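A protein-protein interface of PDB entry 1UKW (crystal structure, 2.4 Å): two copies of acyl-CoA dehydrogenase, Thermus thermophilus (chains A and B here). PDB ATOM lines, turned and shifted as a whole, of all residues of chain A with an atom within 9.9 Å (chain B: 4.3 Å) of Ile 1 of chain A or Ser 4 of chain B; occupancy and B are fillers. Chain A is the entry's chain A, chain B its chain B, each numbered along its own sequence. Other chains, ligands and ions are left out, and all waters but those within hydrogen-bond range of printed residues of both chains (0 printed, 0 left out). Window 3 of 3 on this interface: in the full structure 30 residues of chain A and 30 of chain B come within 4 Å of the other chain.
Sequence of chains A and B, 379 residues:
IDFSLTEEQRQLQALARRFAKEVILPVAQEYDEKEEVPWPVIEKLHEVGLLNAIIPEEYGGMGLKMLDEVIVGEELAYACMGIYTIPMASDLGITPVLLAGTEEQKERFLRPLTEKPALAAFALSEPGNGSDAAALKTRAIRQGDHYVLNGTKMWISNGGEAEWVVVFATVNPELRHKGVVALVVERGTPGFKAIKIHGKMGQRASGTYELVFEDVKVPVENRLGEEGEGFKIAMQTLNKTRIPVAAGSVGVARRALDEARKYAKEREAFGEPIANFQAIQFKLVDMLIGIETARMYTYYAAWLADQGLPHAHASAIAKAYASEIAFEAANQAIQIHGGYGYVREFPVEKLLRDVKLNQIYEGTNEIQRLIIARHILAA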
ATOM      1  N   ILE A   1      23.987  17.634 -25.458  1.00  0.00           N
ATOM      2  CA  ILE A   1      23.498  17.311 -24.076  1.00  0.00           C
ATOM      3  C   ILE A   1      22.935  18.551 -23.361  1.00  0.00           C
ATOM      4  O   ILE A   1      23.607  19.595 -23.269  1.00  0.00           O
ATOM      5  CB  ILE A   1      24.638  16.729 -23.211  1.00  0.00           C
ATOM      6  CG1 ILE A   1      24.067  16.183 -21.893  1.00  0.00           C
ATOM      7  CG2 ILE A   1      25.684  17.822 -22.938  1.00  0.00           C
ATOM      8  CD1 ILE A   1      25.069  15.355 -21.055  1.00  0.00           C
ATOM      9  N   ASP A   2      21.714  18.424 -22.837  1.00  0.00           N
ATOM     10  CA  ASP A   2      21.049  19.531 -22.149  1.00  0.00           C
ATOM     11  C   ASP A   2      19.962  19.008 -21.199  1.00  0.00           C
ATOM     12  O   ASP A   2      18.951  18.472 -21.651  1.00  0.00           O
ATOM     13  CB  ASP A   2      20.423  20.473 -23.189  1.00  0.00           C
ATOM     14  CG  ASP A   2      19.435  21.446 -22.580  1.00  0.00           C
ATOM     15  OD1 ASP A   2      18.620  22.006 -23.347  1.00  0.00           O
ATOM     16  OD2 ASP A   2      19.467  21.658 -21.347  1.00  0.00           O
ATOM     17  N   PHE A   3      20.159  19.190 -19.892  1.00  0.00           N
ATOM     18  CA  PHE A   3      19.197  18.707 -18.897  1.00  0.00           C
ATOM     19  C   PHE A   3      18.121  19.722 -18.502  1.00  0.00           C
ATOM     20  O   PHE A   3      17.152  19.367 -17.811  1.00  0.00           O
ATOM     21  CB  PHE A   3      19.919  18.284 -17.616  1.00  0.00           C
ATOM     22  CG  PHE A   3      21.000  17.259 -17.819  1.00  0.00           C
ATOM     23  CD1 PHE A   3      22.140  17.561 -18.556  1.00  0.00           C
ATOM     24  CD2 PHE A   3      20.918  16.016 -17.196  1.00  0.00           C
ATOM     25  CE1 PHE A   3      23.187  16.649 -18.667  1.00  0.00           C
ATOM     26  CE2 PHE A   3      21.967  15.089 -17.301  1.00  0.00           C
ATOM     27  CZ  PHE A   3      23.107  15.416 -18.042  1.00  0.00           C
ATOM     28  N   SER A   4      18.286  20.972 -18.927  1.00  0.00           N
ATOM     29  CA  SER A   4      17.341  22.038 -18.581  1.00  0.00           C
ATOM     30  C   SER A   4      15.922  21.778 -19.082  1.00  0.00           C
ATOM     31  O   SER A   4      15.691  20.839 -19.857  1.00  0.00           O
ATOM     32  CB  SER A   4      17.843  23.383 -19.119  1.00  0.00           C
ATOM     33  OG  SER A   4      17.336  24.473 -18.347  1.00  0.00           O
ATOM     34  N   TYR A 300      16.452  10.670 -17.083  1.00  0.00           N
ATOM     35  CA  TYR A 300      17.144   9.933 -18.130  1.00  0.00           C
ATOM     36  C   TYR A 300      16.268   8.833 -18.726  1.00  0.00           C
ATOM     37  O   TYR A 300      16.103   8.763 -19.946  1.00  0.00           O
ATOM     38  CB  TYR A 300      18.442   9.333 -17.580  1.00  0.00           C
ATOM     39  CG  TYR A 300      19.182   8.447 -18.556  1.00  0.00           C
ATOM     40  CD1 TYR A 300      19.390   7.093 -18.274  1.00  0.00           C
ATOM     41  CD2 TYR A 300      19.676   8.957 -19.763  1.00  0.00           C
ATOM     42  CE1 TYR A 300      20.070   6.264 -19.162  1.00  0.00           C
ATOM     43  CE2 TYR A 300      20.361   8.132 -20.665  1.00  0.00           C
ATOM     44  CZ  TYR A 300      20.553   6.788 -20.354  1.00  0.00           C
ATOM     45  OH  TYR A 300      21.228   5.965 -21.226  1.00  0.00           O
ATOM     46  N   TRP A 303      13.703  10.155 -20.723  1.00  0.00           N
ATOM     47  CA  TRP A 303      14.247  10.615 -21.989  1.00  0.00           C
ATOM     48  C   TRP A 303      14.308   9.461 -22.989  1.00  0.00           C
ATOM     49  O   TRP A 303      13.887   9.610 -24.133  1.00  0.00           O
ATOM     50  CB  TRP A 303      15.649  11.183 -21.784  1.00  0.00           C
ATOM     51  CG  TRP A 303      16.309  11.583 -23.056  1.00  0.00           C
ATOM     52  CD1 TRP A 303      15.964  12.628 -23.866  1.00  0.00           C
ATOM     53  CD2 TRP A 303      17.425  10.938 -23.683  1.00  0.00           C
ATOM     54  NE1 TRP A 303      16.795  12.674 -24.957  1.00  0.00           N
ATOM     55  CE2 TRP A 303      17.703  11.650 -24.871  1.00  0.00           C
ATOM     56  CE3 TRP A 303      18.215   9.828 -23.356  1.00  0.00           C
ATOM     57  CZ2 TRP A 303      18.741  11.290 -25.737  1.00  0.00           C
ATOM     58  CZ3 TRP A 303      19.253   9.468 -24.218  1.00  0.00           C
ATOM     59  CH2 TRP A 303      19.504  10.199 -25.394  1.00  0.00           C
ATOM     60  N   LEU A 304      14.832   8.316 -22.553  1.00  0.00           N
ATOM     61  CA  LEU A 304      14.940   7.146 -23.424  1.00  0.00           C
ATOM     62  C   LEU A 304      13.568   6.748 -23.955  1.00  0.00           C
ATOM     63  O   LEU A 304      13.420   6.421 -25.129  1.00  0.00           O
ATOM     64  CB  LEU A 304      15.548   5.953 -22.673  1.00  0.00           C
ATOM     65  CG  LEU A 304      16.990   6.004 -22.143  1.00  0.00           C
ATOM     66  CD1 LEU A 304      17.245   4.753 -21.309  1.00  0.00           C
ATOM     67  CD2 LEU A 304      17.997   6.095 -23.300  1.00  0.00           C
ATOM     68  N   GLN A 307      12.434   9.317 -26.509  1.00  0.00           N
ATOM     69  CA  GLN A 307      13.256   9.142 -27.701  1.00  0.00           C
ATOM     70  C   GLN A 307      13.016   7.808 -28.397  1.00  0.00           C
ATOM     71  O   GLN A 307      13.535   7.576 -29.493  1.00  0.00           O
ATOM     72  CB  GLN A 307      14.734   9.255 -27.327  1.00  0.00           C
ATOM     73  CG  GLN A 307      15.105  10.623 -26.796  1.00  0.00           C
ATOM     74  CD  GLN A 307      14.820  11.700 -27.820  1.00  0.00           C
ATOM     75  OE1 GLN A 307      15.305  11.628 -28.955  1.00  0.00           O
ATOM     76  NE2 GLN A 307      14.033  12.700 -27.435  1.00  0.00           N
ATOM     77  N   LEU A 309      14.008   4.815 -27.295  1.00  0.00           N
ATOM     78  CA  LEU A 309      15.142   3.910 -27.107  1.00  0.00           C
ATOM     79  C   LEU A 309      14.842   2.850 -26.048  1.00  0.00           C
ATOM     80  O   LEU A 309      13.887   2.979 -25.286  1.00  0.00           O
ATOM     81  CB  LEU A 309      16.378   4.714 -26.690  1.00  0.00           C
ATOM     82  CG  LEU A 309      16.857   5.766 -27.697  1.00  0.00           C
ATOM     83  CD1 LEU A 309      17.646   6.850 -26.987  1.00  0.00           C
ATOM     84  CD2 LEU A 309      17.696   5.097 -28.781  1.00  0.00           C
ATOM     85  N   ASP B   2      17.993  16.681 -23.030  1.00  0.00           N
ATOM     86  CA  ASP B   2      18.731  15.737 -23.863  1.00  0.00           C
ATOM     87  C   ASP B   2      19.941  15.217 -23.079  1.00  0.00           C
ATOM     88  O   ASP B   2      20.628  15.990 -22.403  1.00  0.00           O
ATOM     89  CB  ASP B   2      19.207  16.446 -25.138  1.00  0.00           C
ATOM     90  CG  ASP B   2      19.919  15.512 -26.099  1.00  0.00           C
ATOM     91  OD1 ASP B   2      20.457  16.008 -27.112  1.00  0.00           O
ATOM     92  OD2 ASP B   2      19.935  14.285 -25.846  1.00  0.00           O
ATOM     93  N   PHE B   3      20.193  13.913 -23.163  1.00  0.00           N
ATOM     94  CA  PHE B   3      21.327  13.297 -22.466  1.00  0.00           C
ATOM     95  C   PHE B   3      22.252  12.631 -23.481  1.00  0.00           C
ATOM     96  O   PHE B   3      23.112  11.826 -23.117  1.00  0.00           O
ATOM     97  CB  PHE B   3      20.858  12.221 -21.482  1.00  0.00           C
ATOM     98  CG  PHE B   3      19.917  12.720 -20.423  1.00  0.00           C
ATOM     99  CD1 PHE B   3      18.589  13.002 -20.727  1.00  0.00           C
ATOM    100  CD2 PHE B   3      20.345  12.859 -19.111  1.00  0.00           C
ATOM    101  CE1 PHE B   3      17.706  13.408 -19.748  1.00  0.00           C
ATOM    102  CE2 PHE B   3      19.459  13.268 -18.116  1.00  0.00           C
ATOM    103  CZ  PHE B   3      18.135  13.541 -18.443  1.00  0.00           C
ATOM    104  N   SER B   4      22.072  12.971 -24.751  1.00  0.00           N
ATOM    105  CA  SER B   4      22.871  12.387 -25.823  1.00  0.00           C
ATOM    106  C   SER B   4      24.237  13.028 -26.046  1.00  0.00           C
ATOM    107  O   SER B   4      24.417  14.237 -25.844  1.00  0.00           O
ATOM    108  CB  SER B   4      22.090  12.445 -27.132  1.00  0.00           C
ATOM    109  OG  SER B   4      22.844  11.848 -28.170  1.00  0.00           O
ATOM    110  N   LEU B   5      25.199  12.205 -26.468  1.00  0.00           N
ATOM    111  CA  LEU B   5      26.544  12.688 -26.768  1.00  0.00           C
ATOM    112  C   LEU B   5      26.539  13.124 -28.218  1.00  0.00           C
ATOM    113  O   LEU B   5      25.799  12.563 -29.032  1.00  0.00           O
ATOM    114  CB  LEU B   5      27.596  11.581 -26.600  1.00  0.00           C
ATOM    115  CG  LEU B   5      28.219  11.362 -25.221  1.00  0.00           C
ATOM    116  CD1 LEU B   5      27.139  10.980 -24.226  1.00  0.00           C
ATOM    117  CD2 LEU B   5      29.281  10.278 -25.313  1.00  0.00           C
ATOM    118  N   THR B   6      27.362  14.115 -28.544  1.00  0.00           N
ATOM    119  CA  THR B   6      27.451  14.588 -29.919  1.00  0.00           C
ATOM    120  C   THR B   6      28.385  13.654 -30.684  1.00  0.00           C
ATOM    121  O   THR B   6      29.038  12.784 -30.092  1.00  0.00           O
ATOM    122  CB  THR B   6      28.021  16.012 -29.997  1.00  0.00           C
ATOM    123  OG1 THR B   6      29.355  16.016 -29.473  1.00  0.00           O
ATOM    124  CG2 THR B   6      27.149  16.983 -29.193  1.00  0.00           C
ATOM    125  N   GLN B   9      31.871  13.844 -29.292  1.00  0.00           N
ATOM    126  CA  GLN B   9      32.016  13.211 -27.989  1.00  0.00           C
ATOM    127  C   GLN B   9      32.188  11.706 -28.134  1.00  0.00           C
ATOM    128  O   GLN B   9      33.060  11.116 -27.496  1.00  0.00           O
ATOM    129  CB  GLN B   9      30.813  13.556 -27.108  1.00  0.00           C
ATOM    130  CG  GLN B   9      30.509  15.046 -27.137  1.00  0.00           C
ATOM    131  CD  GLN B   9      29.529  15.487 -26.073  1.00  0.00           C
ATOM    132  OE1 GLN B   9      28.459  14.891 -25.900  1.00  0.00           O
ATOM    133  NE2 GLN B   9      29.886  16.557 -25.354  1.00  0.00           N
ATOM    134  N   ARG B  10      31.375  11.084 -28.985  1.00  0.00           N
ATOM    135  CA  ARG B  10      31.489   9.647 -29.202  1.00  0.00           C
ATOM    136  C   ARG B  10      32.871   9.312 -29.743  1.00  0.00           C
ATOM    137  O   ARG B  10      33.449   8.274 -29.400  1.00  0.00           O
ATOM    138  CB  ARG B  10      30.424   9.154 -30.183  1.00  0.00           C
ATOM    139  CG  ARG B  10      29.012   9.302 -29.670  1.00  0.00           C
ATOM    140  CD  ARG B  10      28.091   8.293 -30.335  1.00  0.00           C
ATOM    141  NE  ARG B  10      26.683   8.575 -30.075  1.00  0.00           N
ATOM    142  CZ  ARG B  10      26.062   9.677 -30.491  1.00  0.00           C
ATOM    143  NH1 ARG B  10      26.733  10.597 -31.182  1.00  0.00           N
ATOM    144  NH2 ARG B  10      24.766   9.853 -30.235  1.00  0.00           N
ATOM    145  N   LEU B  67      32.069  18.043 -19.524  1.00  0.00           N
ATOM    146  CA  LEU B  67      31.339  16.882 -20.009  1.00  0.00           C
ATOM    147  C   LEU B  67      32.339  15.967 -20.710  1.00  0.00           C
ATOM    148  O   LEU B  67      32.299  14.744 -20.555  1.00  0.00           O
ATOM    149  CB  LEU B  67      30.254  17.311 -20.993  1.00  0.00           C
ATOM    150  CG  LEU B  67      29.492  16.164 -21.667  1.00  0.00           C
ATOM    151  CD1 LEU B  67      28.680  15.362 -20.638  1.00  0.00           C
ATOM    152  CD2 LEU B  67      28.595  16.745 -22.737  1.00  0.00           C
ATOM    153  N   TRP B 303      27.379  19.102 -16.670  1.00  0.00           N
ATOM    154  CA  TRP B 303      26.524  19.978 -17.450  1.00  0.00           C
ATOM    155  C   TRP B 303      26.410  21.333 -16.755  1.00  0.00           C
ATOM    156  O   TRP B 303      26.619  22.369 -17.375  1.00  0.00           O
ATOM    157  CB  TRP B 303      25.127  19.365 -17.597  1.00  0.00           C
ATOM    158  CG  TRP B 303      24.162  20.256 -18.327  1.00  0.00           C
ATOM    159  CD1 TRP B 303      24.163  20.544 -19.659  1.00  0.00           C
ATOM    160  CD2 TRP B 303      23.066  20.985 -17.757  1.00  0.00           C
ATOM    161  NE1 TRP B 303      23.133  21.408 -19.958  1.00  0.00           N
ATOM    162  CE2 TRP B 303      22.445  21.696 -18.809  1.00  0.00           C
ATOM    163  CE3 TRP B 303      22.547  21.107 -16.460  1.00  0.00           C
ATOM    164  CZ2 TRP B 303      21.323  22.519 -18.604  1.00  0.00           C
ATOM    165  CZ3 TRP B 303      21.431  21.925 -16.256  1.00  0.00           C
ATOM    166  CH2 TRP B 303      20.834  22.620 -17.325  1.00  0.00           C
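Asp 2 of chain B touches Ile 1 of chain A (O to CG1, 3.5 Å). CG2 of Ile 1 of chain A touches CD2 of Leu 67 of chain B (3.1 Å). O of Ile 1 of chain A touches CD1 of Trp 303 of chain B, 3.8 Å away. CZ2 of Trp 303 of chain B touches OD2 of Asp 2 of chain A (3.4 Å). Phe 3 of chain A touches Phe 3 of chain B. Phe 3 of chain A touches Trp 303 of chain B (CD1 to CG, 3.4 Å). Ser 4 of chain A touches Trp 303 of chain B (N to CZ2, 3.4 Å). Phe 3 of chain B touches Tyr 300 of chain A (CZ to N, 3.6 Å). CD1 of Phe 3 of chain B touches CG of Trp 303 of chain A, 3.6 Å away. Ser 4 of chain B touches Trp 303 of chain A.
Of chain B, only Asp 2 (3.5 Å), Ser 4 (3.4 Å), Leu 67 (3.1 Å) and Trp 303 (3.8 Å) come within 4 Å of Ile 1 of chain A. Ser 4 of chain B touches just these residues of chain A: Ile 1 and Trp 303. Of chain A, only Ile 1, Asp 2 and Trp 303 come within 4 Å of Asp 2 of chain B. Leu 5 of chain B touches none of the printed residues of chain A. Of the printed residues of chain A, Phe 3 of chain B touches Phe 3, Tyr 300 and Trp 303. Of the printed residues of chain B, Phe 3 of chain A touches Phe 3 and Trp 303. The nearest residue of chain B that does not touch Ile 1 of chain A is Phe 3 of chain B (4.02 Å).
The guanidinium group (NH2) of Arg 10 of chain B sits at hydrogen-bond distance from the side-chain hydroxyl (OG) of Ser 4 of chain B (3.5 Å). N of Ser 4 of chain B sits at hydrogen-bond distance from OD2 of Asp 2 of chain B (2.7 Å). OD2 of Asp 2 of chain A is in hydrogen-bond range of N of Ser 4 of chain A (2.8 Å).
Hydrophobic or aromatic side chains of chain A within 4 Å of the printed part of chain B: Ile 1, Phe 3, Tyr 300 and Trp 303. Of the 9 printed residues of chain B, 5 touch a printed residue of chain A. Among the printed residues, no Asp or Glu carboxylate lies within 4 Å of a Lys or Arg side-chain nitrogen of the other chain.
N of Ile 1 of chain A lies within hydrogen-bond range of O of Ser 4 of chain B, 3.4 Å away. The backbone carbonyl oxygen (O) of Asp 2 of chain A is in hydrogen-bond range of the backbone NH (N) of Asp 2 of chain B, 2.5 Å away.
Asp 2 of chain A touches its own counterpart, Asp 2 of chain B. Asp 2 of chain A touches Trp 303 of chain B, and with the chains exchanged Trp 303 of chain A touches Asp 2 of chain B. Phe 3 of chain B touches its own counterpart, Phe 3 of chain A. Ser 4 of chain A touches Trp 303 of chain B, and with the chains exchanged Trp 303 of chain A touches Ser 4 of chain B. Positions printed for both chains: 2, 3, 4 and 303. Of the 13 pairs that touch across the chains among the printed residues, 8 have their exchanged pair printed and touching as well.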
